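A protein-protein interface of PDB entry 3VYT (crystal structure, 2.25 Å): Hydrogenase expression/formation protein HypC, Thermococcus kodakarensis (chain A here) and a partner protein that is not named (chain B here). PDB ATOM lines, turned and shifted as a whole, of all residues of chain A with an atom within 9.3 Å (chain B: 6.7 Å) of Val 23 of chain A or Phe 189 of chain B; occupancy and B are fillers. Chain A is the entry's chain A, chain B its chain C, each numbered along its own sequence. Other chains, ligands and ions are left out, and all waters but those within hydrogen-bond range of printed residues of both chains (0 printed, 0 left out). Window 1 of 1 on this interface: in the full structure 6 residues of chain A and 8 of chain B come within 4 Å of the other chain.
The backbone NH of Gly 21 of chain A lies within hydrogen-bond range of the side-chain carboxylate of Asp 19 of chain A (3.1 Å).
The backbone NH (N) of Val 23 of chain A is in hydrogen-bond range of the side-chain carboxylate (OD2) of Asp 19 of chain A (3.1 Å).
The backbone carbonyl oxygen (O) of Ser 182 of chain B is in hydrogen-bond range of the backbone NH (N) of Ile 187 of chain B.
The backbone carbonyl oxygen of Val 18 of chain A lies within hydrogen-bond range of the backbone NH of Arg 25 of chain A (2.9 Å).
The side-chain carboxylate of Asp 19 of chain A is in hydrogen-bond range of the backbone NH of Gly 22 of chain A.
Val 23 of chain A touches just these residues of chain B: Ile 187 (3.3 Å), Ala 188 (3.7 Å), Phe 189 (3.1 Å), Glu 254 (3.7 Å), Ala 257 (3.9 Å) and Met 261 (3.3 Å).
Phe 189 of chain B touches just these residues of chain A: Gly 22 and Val 23.
Of the printed residues of chain A, Ala 188 of chain B touches Val 23 (3.7 Å) and Lys 24 (3.0 Å).
Of the printed residues of chain B, Arg 25 of chain A touches Ile 187 (3.2 Å) and Met 261 (3.4 Å).
Printed residues of chain B within 4 Å of Gly 21 of chain A: Pro 253 (3.8 Å), Glu 254 (3.6 Å) and Ala 257 (3.97 Å).
Ile 178 of chain B touches none of the printed residues of chain A.
Ile 9 of chain A touches none of the printed residues of chain B.
The nearest residue of chain B that does not touch Val 23 of chain A is Ala 258 of chain B (4.2 Å).
The nearest residue of chain A that does not touch Phe 189 of chain B is Lys 24 of chain A (4.4 Å).
O of Gly 22 of chain A lies within hydrogen-bond range of N of Glu 190 of chain B.
The backbone NH (N) of Lys 24 of chain A sits at hydrogen-bond distance from the backbone carbonyl oxygen (O) of Ala 188 of chain B, 3.0 Å away.
Of the 17 printed residues of chain A, 6 touch a printed residue of chain B.
Hydrophobic or aromatic side chains of chain A within 4 Å of the printed part of chain B: Phe 20 and Val 23.
Of the 18 printed residues of chain B, 8 touch a printed residue of chain A.
Hydrophobic or aromatic side chains of chain B that line the printed part of chain A: Ile 187, Phe 189, Ala 257 and Met 261.
Ala 257 of chain B touches Phe 20 of chain A.
Phe 20 of chain A touches Met 261 of chain B.
O of Gly 21 of chain A touches CA of Glu 254 of chain B (3.6 Å).
CB of Ala 257 of chain B touches O of Gly 21 of chain A (3.97 Å).
Gly 22 of chain A touches Phe 189 of chain B (O to CD1, 3.0 Å).
Val 23 of chain A touches Glu 254 of chain B (CG2 to O, 3.7 Å).
Val 23 of chain A touches Ala 257 of chain B.
CG1 of Val 23 of chain A touches CE of Met 261 of chain B, at 3.3 Å.
Lys 24 of chain A touches Glu 190 of chain B.
Arg 25 of chain A touches Met 261 of chain B.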
ATOM      1  N   VAL A   4     -24.498  -1.752  30.526  1.00  0.00           N
ATOM      2  CA  VAL A   4     -23.193  -1.387  29.975  1.00  0.00           C
ATOM      3  C   VAL A   4     -23.152  -1.552  28.441  1.00  0.00           C
ATOM      4  O   VAL A   4     -23.861  -2.392  27.872  1.00  0.00           O
ATOM      5  CB  VAL A   4     -22.069  -2.237  30.652  1.00  0.00           C
ATOM      6  CG1 VAL A   4     -22.428  -3.713  30.595  1.00  0.00           C
ATOM      7  CG2 VAL A   4     -20.717  -1.981  29.985  1.00  0.00           C
ATOM      8  N   PRO A   5     -22.335  -0.731  27.753  1.00  0.00           N
ATOM      9  CA  PRO A   5     -22.190  -0.765  26.292  1.00  0.00           C
ATOM     10  C   PRO A   5     -21.388  -1.953  25.773  1.00  0.00           C
ATOM     11  O   PRO A   5     -20.420  -2.389  26.397  1.00  0.00           O
ATOM     12  CB  PRO A   5     -21.486   0.556  25.977  1.00  0.00           C
ATOM     13  CG  PRO A   5     -21.828   1.433  27.144  1.00  0.00           C
ATOM     14  CD  PRO A   5     -21.703   0.482  28.298  1.00  0.00           C
ATOM     15  N   GLY A   6     -21.787  -2.459  24.614  1.00  0.00           N
ATOM     16  CA  GLY A   6     -21.093  -3.585  24.025  1.00  0.00           C
ATOM     17  C   GLY A   6     -21.152  -3.519  22.514  1.00  0.00           C
ATOM     18  O   GLY A   6     -22.098  -2.973  21.946  1.00  0.00           O
ATOM     19  N   LYS A   7     -20.138  -4.079  21.863  1.00  0.00           N
ATOM     20  CA  LYS A   7     -20.068  -4.083  20.411  1.00  0.00           C
ATOM     21  C   LYS A   7     -20.580  -5.402  19.858  1.00  0.00           C
ATOM     22  O   LYS A   7     -20.070  -6.469  20.206  1.00  0.00           O
ATOM     23  CB  LYS A   7     -18.625  -3.870  19.949  1.00  0.00           C
ATOM     24  CG  LYS A   7     -18.466  -3.745  18.441  1.00  0.00           C
ATOM     25  CD  LYS A   7     -17.001  -3.622  18.039  1.00  0.00           C
ATOM     26  CE  LYS A   7     -16.277  -4.969  18.089  1.00  0.00           C
ATOM     27  NZ  LYS A   7     -16.266  -5.605  19.437  1.00  0.00           N
ATOM     28  N   VAL A   8     -21.588  -5.322  18.998  1.00  0.00           N
ATOM     29  CA  VAL A   8     -22.158  -6.506  18.386  1.00  0.00           C
ATOM     30  C   VAL A   8     -21.173  -7.124  17.401  1.00  0.00           C
ATOM     31  O   VAL A   8     -20.636  -6.441  16.531  1.00  0.00           O
ATOM     32  CB  VAL A   8     -23.449  -6.164  17.646  1.00  0.00           C
ATOM     33  CG1 VAL A   8     -23.915  -7.355  16.828  1.00  0.00           C
ATOM     34  CG2 VAL A   8     -24.511  -5.759  18.645  1.00  0.00           C
ATOM     35  N   ILE A   9     -20.938  -8.423  17.546  1.00  0.00           N
ATOM     36  CA  ILE A   9     -20.019  -9.124  16.663  1.00  0.00           C
ATOM     37  C   ILE A   9     -20.680 -10.328  16.003  1.00  0.00           C
ATOM     38  O   ILE A   9     -19.996 -11.161  15.417  1.00  0.00           O
ATOM     39  CB  ILE A   9     -18.769  -9.610  17.427  1.00  0.00           C
ATOM     40  CG1 ILE A   9     -19.157 -10.692  18.433  1.00  0.00           C
ATOM     41  CG2 ILE A   9     -18.109  -8.444  18.140  1.00  0.00           C
ATOM     42  CD1 ILE A   9     -17.970 -11.316  19.145  1.00  0.00           C
ATOM     43  N   VAL A  17     -24.415 -11.623  19.609  1.00  0.00           N
ATOM     44  CA  VAL A  17     -23.243 -11.832  20.456  1.00  0.00           C
ATOM     45  C   VAL A  17     -22.491 -10.515  20.633  1.00  0.00           C
ATOM     46  O   VAL A  17     -21.826 -10.031  19.710  1.00  0.00           O
ATOM     47  CB  VAL A  17     -22.287 -12.880  19.857  1.00  0.00           C
ATOM     48  CG1 VAL A  17     -21.084 -13.058  20.762  1.00  0.00           C
ATOM     49  CG2 VAL A  17     -23.016 -14.198  19.673  1.00  0.00           C
ATOM     50  N   VAL A  18     -22.598  -9.950  21.832  1.00  0.00           N
ATOM     51  CA  VAL A  18     -21.967  -8.682  22.148  1.00  0.00           C
ATOM     52  C   VAL A  18     -20.670  -8.853  22.936  1.00  0.00           C
ATOM     53  O   VAL A  18     -20.558  -9.724  23.796  1.00  0.00           O
ATOM     54  CB  VAL A  18     -22.945  -7.799  22.950  1.00  0.00           C
ATOM     55  CG1 VAL A  18     -22.384  -6.403  23.110  1.00  0.00           C
ATOM     56  CG2 VAL A  18     -24.297  -7.757  22.246  1.00  0.00           C
ATOM     57  N   ASP A  19     -19.685  -8.020  22.626  1.00  0.00           N
ATOM     58  CA  ASP A  19     -18.401  -8.069  23.314  1.00  0.00           C
ATOM     59  C   ASP A  19     -18.264  -6.832  24.178  1.00  0.00           C
ATOM     60  O   ASP A  19     -18.334  -5.704  23.684  1.00  0.00           O
ATOM     61  CB  ASP A  19     -17.239  -8.116  22.313  1.00  0.00           C
ATOM     62  CG  ASP A  19     -15.866  -8.117  22.996  1.00  0.00           C
ATOM     63  OD1 ASP A  19     -14.849  -8.007  22.278  1.00  0.00           O
ATOM     64  OD2 ASP A  19     -15.797  -8.230  24.244  1.00  0.00           O
ATOM     65  N   PHE A  20     -18.087  -7.048  25.476  1.00  0.00           N
ATOM     66  CA  PHE A  20     -17.918  -5.948  26.404  1.00  0.00           C
ATOM     67  C   PHE A  20     -16.470  -5.948  26.862  1.00  0.00           C
ATOM     68  O   PHE A  20     -16.168  -6.275  28.005  1.00  0.00           O
ATOM     69  CB  PHE A  20     -18.849  -6.101  27.606  1.00  0.00           C
ATOM     70  CG  PHE A  20     -20.296  -6.232  27.237  1.00  0.00           C
ATOM     71  CD1 PHE A  20     -20.828  -7.465  26.874  1.00  0.00           C
ATOM     72  CD2 PHE A  20     -21.132  -5.121  27.245  1.00  0.00           C
ATOM     73  CE1 PHE A  20     -22.175  -7.590  26.523  1.00  0.00           C
ATOM     74  CE2 PHE A  20     -22.483  -5.235  26.895  1.00  0.00           C
ATOM     75  CZ  PHE A  20     -23.004  -6.471  26.534  1.00  0.00           C
ATOM     76  N   GLY A  21     -15.569  -5.605  25.950  1.00  0.00           N
ATOM     77  CA  GLY A  21     -14.162  -5.561  26.288  1.00  0.00           C
ATOM     78  C   GLY A  21     -13.574  -6.893  26.706  1.00  0.00           C
ATOM     79  O   GLY A  21     -13.131  -7.054  27.843  1.00  0.00           O
ATOM     80  N   GLY A  22     -13.565  -7.854  25.790  1.00  0.00           N
ATOM     81  CA  GLY A  22     -12.992  -9.153  26.099  1.00  0.00           C
ATOM     82  C   GLY A  22     -13.938 -10.120  26.780  1.00  0.00           C
ATOM     83  O   GLY A  22     -13.546 -11.227  27.150  1.00  0.00           O
ATOM     84  N   VAL A  23     -15.183  -9.693  26.956  1.00  0.00           N
ATOM     85  CA  VAL A  23     -16.206 -10.521  27.584  1.00  0.00           C
ATOM     86  C   VAL A  23     -17.415 -10.517  26.662  1.00  0.00           C
ATOM     87  O   VAL A  23     -18.000  -9.468  26.404  1.00  0.00           O
ATOM     88  CB  VAL A  23     -16.632  -9.960  28.957  1.00  0.00           C
ATOM     89  CG1 VAL A  23     -17.715 -10.841  29.560  1.00  0.00           C
ATOM     90  CG2 VAL A  23     -15.431  -9.872  29.885  1.00  0.00           C
ATOM     91  N   LYS A  24     -17.787 -11.689  26.164  1.00  0.00           N
ATOM     92  CA  LYS A  24     -18.915 -11.785  25.251  1.00  0.00           C
ATOM     93  C   LYS A  24     -20.113 -12.439  25.905  1.00  0.00           C
ATOM     94  O   LYS A  24     -19.958 -13.302  26.766  1.00  0.00           O
ATOM     95  CB  LYS A  24     -18.505 -12.578  24.012  1.00  0.00           C
ATOM     96  CG  LYS A  24     -17.272 -12.024  23.326  1.00  0.00           C
ATOM     97  CD  LYS A  24     -16.857 -12.879  22.143  1.00  0.00           C
ATOM     98  CE  LYS A  24     -15.611 -12.322  21.474  1.00  0.00           C
ATOM     99  NZ  LYS A  24     -15.238 -13.121  20.278  1.00  0.00           N
ATOM    100  N   ARG A  25     -21.307 -12.018  25.489  1.00  0.00           N
ATOM    101  CA  ARG A  25     -22.559 -12.560  26.009  1.00  0.00           C
ATOM    102  C   ARG A  25     -23.644 -12.499  24.936  1.00  0.00           C
ATOM    103  O   ARG A  25     -23.607 -11.633  24.062  1.00  0.00           O
ATOM    104  CB  ARG A  25     -23.013 -11.767  27.237  1.00  0.00           C
ATOM    105  CG  ARG A  25     -22.027 -11.794  28.391  1.00  0.00           C
ATOM    106  CD  ARG A  25     -22.623 -11.189  29.652  1.00  0.00           C
ATOM    107  NE  ARG A  25     -23.843 -11.874  30.074  1.00  0.00           N
ATOM    108  CZ  ARG A  25     -23.913 -13.161  30.403  1.00  0.00           C
ATOM    109  NH1 ARG A  25     -22.828 -13.925  30.365  1.00  0.00           N
ATOM    110  NH2 ARG A  25     -25.075 -13.685  30.770  1.00  0.00           N
ATOM    111  N   GLU A  26     -24.608 -13.416  25.000  1.00  0.00           N
ATOM    112  CA  GLU A  26     -25.696 -13.431  24.025  1.00  0.00           C
ATOM    113  C   GLU A  26     -26.803 -12.474  24.443  1.00  0.00           C
ATOM    114  O   GLU A  26     -27.138 -12.376  25.618  1.00  0.00           O
ATOM    115  CB  GLU A  26     -26.262 -14.845  23.861  1.00  0.00           C
ATOM    116  CG  GLU A  26     -25.276 -15.837  23.259  1.00  0.00           C
ATOM    117  CD  GLU A  26     -25.932 -17.140  22.837  1.00  0.00           C
ATOM    118  OE1 GLU A  26     -26.840 -17.098  21.979  1.00  0.00           O
ATOM    119  OE2 GLU A  26     -25.539 -18.205  23.357  1.00  0.00           O
ATOM    120  N   VAL A  27     -27.376 -11.777  23.469  1.00  0.00           N
ATOM    121  CA  VAL A  27     -28.426 -10.805  23.742  1.00  0.00           C
ATOM    122  C   VAL A  27     -29.595 -10.911  22.766  1.00  0.00           C
ATOM    123  O   VAL A  27     -29.393 -11.113  21.572  1.00  0.00           O
ATOM    124  CB  VAL A  27     -27.861  -9.369  23.648  1.00  0.00           C
ATOM    125  CG1 VAL A  27     -28.918  -8.365  24.057  1.00  0.00           C
ATOM    126  CG2 VAL A  27     -26.612  -9.240  24.514  1.00  0.00           C
ATOM    127  N   ILE B 178     -12.540 -12.250  40.052  1.00  0.00           N
ATOM    128  CA  ILE B 178     -13.425 -12.031  38.910  1.00  0.00           C
ATOM    129  C   ILE B 178     -13.372 -13.200  37.928  1.00  0.00           C
ATOM    130  O   ILE B 178     -14.391 -13.590  37.370  1.00  0.00           O
ATOM    131  CB  ILE B 178     -13.076 -10.721  38.163  1.00  0.00           C
ATOM    132  CG1 ILE B 178     -13.238  -9.526  39.101  1.00  0.00           C
ATOM    133  CG2 ILE B 178     -13.991 -10.540  36.968  1.00  0.00           C
ATOM    134  CD1 ILE B 178     -14.632  -9.381  39.682  1.00  0.00           C
ATOM    135  N   ALA B 179     -12.186 -13.758  37.726  1.00  0.00           N
ATOM    136  CA  ALA B 179     -12.029 -14.892  36.822  1.00  0.00           C
ATOM    137  C   ALA B 179     -12.863 -16.059  37.340  1.00  0.00           C
ATOM    138  O   ALA B 179     -13.601 -16.703  36.592  1.00  0.00           O
ATOM    139  CB  ALA B 179     -10.554 -15.299  36.734  1.00  0.00           C
ATOM    140  N   SER B 182     -16.635 -15.237  37.002  1.00  0.00           N
ATOM    141  CA  SER B 182     -17.022 -15.304  35.607  1.00  0.00           C
ATOM    142  C   SER B 182     -17.118 -16.764  35.170  1.00  0.00           C
ATOM    143  O   SER B 182     -18.025 -17.142  34.433  1.00  0.00           O
ATOM    144  CB  SER B 182     -15.994 -14.562  34.754  1.00  0.00           C
ATOM    145  OG  SER B 182     -15.885 -13.212  35.171  1.00  0.00           O
ATOM    146  N   HIS B 183     -16.175 -17.578  35.634  1.00  0.00           N
ATOM    147  CA  HIS B 183     -16.142 -18.999  35.304  1.00  0.00           C
ATOM    148  C   HIS B 183     -17.406 -19.693  35.803  1.00  0.00           C
ATOM    149  O   HIS B 183     -17.890 -20.638  35.187  1.00  0.00           O
ATOM    150  CB  HIS B 183     -14.909 -19.644  35.944  1.00  0.00           C
ATOM    151  CG  HIS B 183     -14.807 -21.124  35.726  1.00  0.00           C
ATOM    152  ND1 HIS B 183     -14.444 -21.678  34.517  1.00  0.00           N
ATOM    153  CD2 HIS B 183     -15.009 -22.163  36.570  1.00  0.00           C
ATOM    154  CE1 HIS B 183     -14.423 -22.994  34.627  1.00  0.00           C
ATOM    155  NE2 HIS B 183     -14.762 -23.315  35.862  1.00  0.00           N
ATOM    156  N   GLY B 186     -20.711 -18.900  33.743  1.00  0.00           N
ATOM    157  CA  GLY B 186     -20.484 -19.219  32.345  1.00  0.00           C
ATOM    158  C   GLY B 186     -20.088 -18.063  31.446  1.00  0.00           C
ATOM    159  O   GLY B 186     -19.978 -18.237  30.232  1.00  0.00           O
ATOM    160  N   ILE B 187     -19.878 -16.885  32.026  1.00  0.00           N
ATOM    161  CA  ILE B 187     -19.487 -15.714  31.249  1.00  0.00           C
ATOM    162  C   ILE B 187     -18.226 -15.992  30.430  1.00  0.00           C
ATOM    163  O   ILE B 187     -17.118 -16.019  30.965  1.00  0.00           O
ATOM    164  CB  ILE B 187     -19.258 -14.493  32.176  1.00  0.00           C
ATOM    165  CG1 ILE B 187     -20.612 -13.945  32.641  1.00  0.00           C
ATOM    166  CG2 ILE B 187     -18.446 -13.426  31.461  1.00  0.00           C
ATOM    167  CD1 ILE B 187     -20.526 -12.682  33.475  1.00  0.00           C
ATOM    168  N   ALA B 188     -18.411 -16.199  29.127  1.00  0.00           N
ATOM    169  CA  ALA B 188     -17.312 -16.490  28.208  1.00  0.00           C
ATOM    170  C   ALA B 188     -16.543 -15.238  27.786  1.00  0.00           C
ATOM    171  O   ALA B 188     -17.098 -14.141  27.734  1.00  0.00           O
ATOM    172  CB  ALA B 188     -17.850 -17.212  26.973  1.00  0.00           C
ATOM    173  N   PHE B 189     -15.265 -15.417  27.470  1.00  0.00           N
ATOM    174  CA  PHE B 189     -14.407 -14.308  27.061  1.00  0.00           C
ATOM    175  C   PHE B 189     -13.834 -14.479  25.652  1.00  0.00           C
ATOM    176  O   PHE B 189     -13.865 -15.569  25.080  1.00  0.00           O
ATOM    177  CB  PHE B 189     -13.235 -14.171  28.037  1.00  0.00           C
ATOM    178  CG  PHE B 189     -13.627 -13.710  29.405  1.00  0.00           C
ATOM    179  CD1 PHE B 189     -13.207 -12.470  29.874  1.00  0.00           C
ATOM    180  CD2 PHE B 189     -14.401 -14.513  30.233  1.00  0.00           C
ATOM    181  CE1 PHE B 189     -13.550 -12.035  31.153  1.00  0.00           C
ATOM    182  CE2 PHE B 189     -14.752 -14.089  31.514  1.00  0.00           C
ATOM    183  CZ  PHE B 189     -14.324 -12.847  31.975  1.00  0.00           C
ATOM    184  N   GLU B 190     -13.311 -13.386  25.100  1.00  0.00           N
ATOM    185  CA  GLU B 190     -12.670 -13.414  23.791  1.00  0.00           C
ATOM    186  C   GLU B 190     -11.460 -14.329  23.999  1.00  0.00           C
ATOM    187  O   GLU B 190     -11.046 -15.070  23.107  1.00  0.00           O
ATOM    188  CB  GLU B 190     -12.226 -12.001  23.409  1.00  0.00           C
ATOM    189  CG  GLU B 190     -11.117 -11.932  22.378  1.00  0.00           C
ATOM    190  CD  GLU B 190     -10.714 -10.504  22.067  1.00  0.00           C
ATOM    191  OE1 GLU B 190     -10.972  -9.619  22.912  1.00  0.00           O
ATOM    192  OE2 GLU B 190     -10.131 -10.267  20.987  1.00  0.00           O
ATOM    193  N   THR B 191     -10.909 -14.244  25.208  1.00  0.00           N
ATOM    194  CA  THR B 191      -9.781 -15.051  25.680  1.00  0.00           C
ATOM    195  C   THR B 191     -10.071 -15.131  27.185  1.00  0.00           C
ATOM    196  O   THR B 191     -10.217 -14.103  27.848  1.00  0.00           O
ATOM    197  CB  THR B 191      -8.404 -14.361  25.437  1.00  0.00           C
ATOM    198  OG1 THR B 191      -7.953 -13.734  26.643  1.00  0.00           O
ATOM    199  CG2 THR B 191      -8.512 -13.310  24.341  1.00  0.00           C
ATOM    200  N   GLU B 192     -10.186 -16.345  27.718  1.00  0.00           N
ATOM    201  CA  GLU B 192     -10.513 -16.526  29.130  1.00  0.00           C
ATOM    202  C   GLU B 192      -9.717 -15.686  30.116  1.00  0.00           C
ATOM    203  O   GLU B 192      -8.498 -15.546  30.003  1.00  0.00           O
ATOM    204  CB  GLU B 192     -10.391 -18.002  29.538  1.00  0.00           C
ATOM    205  CG  GLU B 192      -8.993 -18.598  29.407  1.00  0.00           C
ATOM    206  CD  GLU B 192      -8.858 -19.922  30.142  1.00  0.00           C
ATOM    207  OE1 GLU B 192      -9.812 -20.727  30.094  1.00  0.00           O
ATOM    208  OE2 GLU B 192      -7.801 -20.162  30.760  1.00  0.00           O
ATOM    209  N   LEU B 193     -10.436 -15.130  31.086  1.00  0.00           N
ATOM    210  CA  LEU B 193      -9.834 -14.330  32.136  1.00  0.00           C
ATOM    211  C   LEU B 193      -9.264 -15.393  33.069  1.00  0.00           C
ATOM    212  O   LEU B 193      -9.991 -16.280  33.518  1.00  0.00           O
ATOM    213  CB  LEU B 193     -10.908 -13.522  32.864  1.00  0.00           C
ATOM    214  CG  LEU B 193     -10.540 -12.194  33.534  1.00  0.00           C
ATOM    215  CD1 LEU B 193     -11.659 -11.809  34.495  1.00  0.00           C
ATOM    216  CD2 LEU B 193      -9.224 -12.310  34.283  1.00  0.00           C
ATOM    217  N   PRO B 253      -8.821  -4.891  31.243  1.00  0.00           N
ATOM    218  CA  PRO B 253     -10.081  -4.538  30.577  1.00  0.00           C
ATOM    219  C   PRO B 253     -11.141  -5.605  30.827  1.00  0.00           C
ATOM    220  O   PRO B 253     -12.298  -5.289  31.116  1.00  0.00           O
ATOM    221  CB  PRO B 253      -9.684  -4.462  29.108  1.00  0.00           C
ATOM    222  CG  PRO B 253      -8.247  -4.028  29.168  1.00  0.00           C
ATOM    223  CD  PRO B 253      -7.701  -4.884  30.285  1.00  0.00           C
ATOM    224  N   GLU B 254     -10.728  -6.867  30.731  1.00  0.00           N
ATOM    225  CA  GLU B 254     -11.625  -8.000  30.933  1.00  0.00           C
ATOM    226  C   GLU B 254     -12.195  -7.990  32.341  1.00  0.00           C
ATOM    227  O   GLU B 254     -13.363  -8.316  32.547  1.00  0.00           O
ATOM    228  CB  GLU B 254     -10.889  -9.328  30.704  1.00  0.00           C
ATOM    229  CG  GLU B 254      -9.939  -9.338  29.518  1.00  0.00           C
ATOM    230  CD  GLU B 254      -8.530  -8.909  29.897  1.00  0.00           C
ATOM    231  OE1 GLU B 254      -7.786  -9.741  30.457  1.00  0.00           O
ATOM    232  OE2 GLU B 254      -8.169  -7.738  29.645  1.00  0.00           O
ATOM    233  N   VAL B 255     -11.361  -7.624  33.310  1.00  0.00           N
ATOM    234  CA  VAL B 255     -11.785  -7.579  34.708  1.00  0.00           C
ATOM    235  C   VAL B 255     -12.769  -6.439  34.948  1.00  0.00           C
ATOM    236  O   VAL B 255     -13.768  -6.616  35.643  1.00  0.00           O
ATOM    237  CB  VAL B 255     -10.571  -7.429  35.660  1.00  0.00           C
ATOM    238  CG1 VAL B 255     -11.045  -7.302  37.096  1.00  0.00           C
ATOM    239  CG2 VAL B 255      -9.654  -8.631  35.513  1.00  0.00           C
ATOM    240  N   ALA B 257     -14.763  -5.101  32.802  1.00  0.00           N
ATOM    241  CA  ALA B 257     -15.984  -5.515  32.128  1.00  0.00           C
ATOM    242  C   ALA B 257     -16.807  -6.534  32.907  1.00  0.00           C
ATOM    243  O   ALA B 257     -18.003  -6.341  33.127  1.00  0.00           O
ATOM    244  CB  ALA B 257     -15.637  -6.067  30.761  1.00  0.00           C
ATOM    245  N   ALA B 258     -16.162  -7.618  33.325  1.00  0.00           N
ATOM    246  CA  ALA B 258     -16.847  -8.670  34.064  1.00  0.00           C
ATOM    247  C   ALA B 258     -17.347  -8.188  35.417  1.00  0.00           C
ATOM    248  O   ALA B 258     -18.425  -8.586  35.867  1.00  0.00           O
ATOM    249  CB  ALA B 258     -15.924  -9.873  34.245  1.00  0.00           C
ATOM    250  N   MET B 261     -20.621  -6.247  34.905  1.00  0.00           N
ATOM    251  CA  MET B 261     -21.708  -7.178  34.639  1.00  0.00           C
ATOM    252  C   MET B 261     -22.055  -7.938  35.911  1.00  0.00           C
ATOM    253  O   MET B 261     -23.229  -8.212  36.186  1.00  0.00           O
ATOM    254  CB  MET B 261     -21.296  -8.162  33.548  1.00  0.00           C
ATOM    255  CG  MET B 261     -21.233  -7.546  32.170  1.00  0.00           C
ATOM    256  SD  MET B 261     -20.625  -8.708  30.949  1.00  0.00           S
ATOM    257  CE  MET B 261     -19.056  -7.983  30.563  1.00  0.00           C
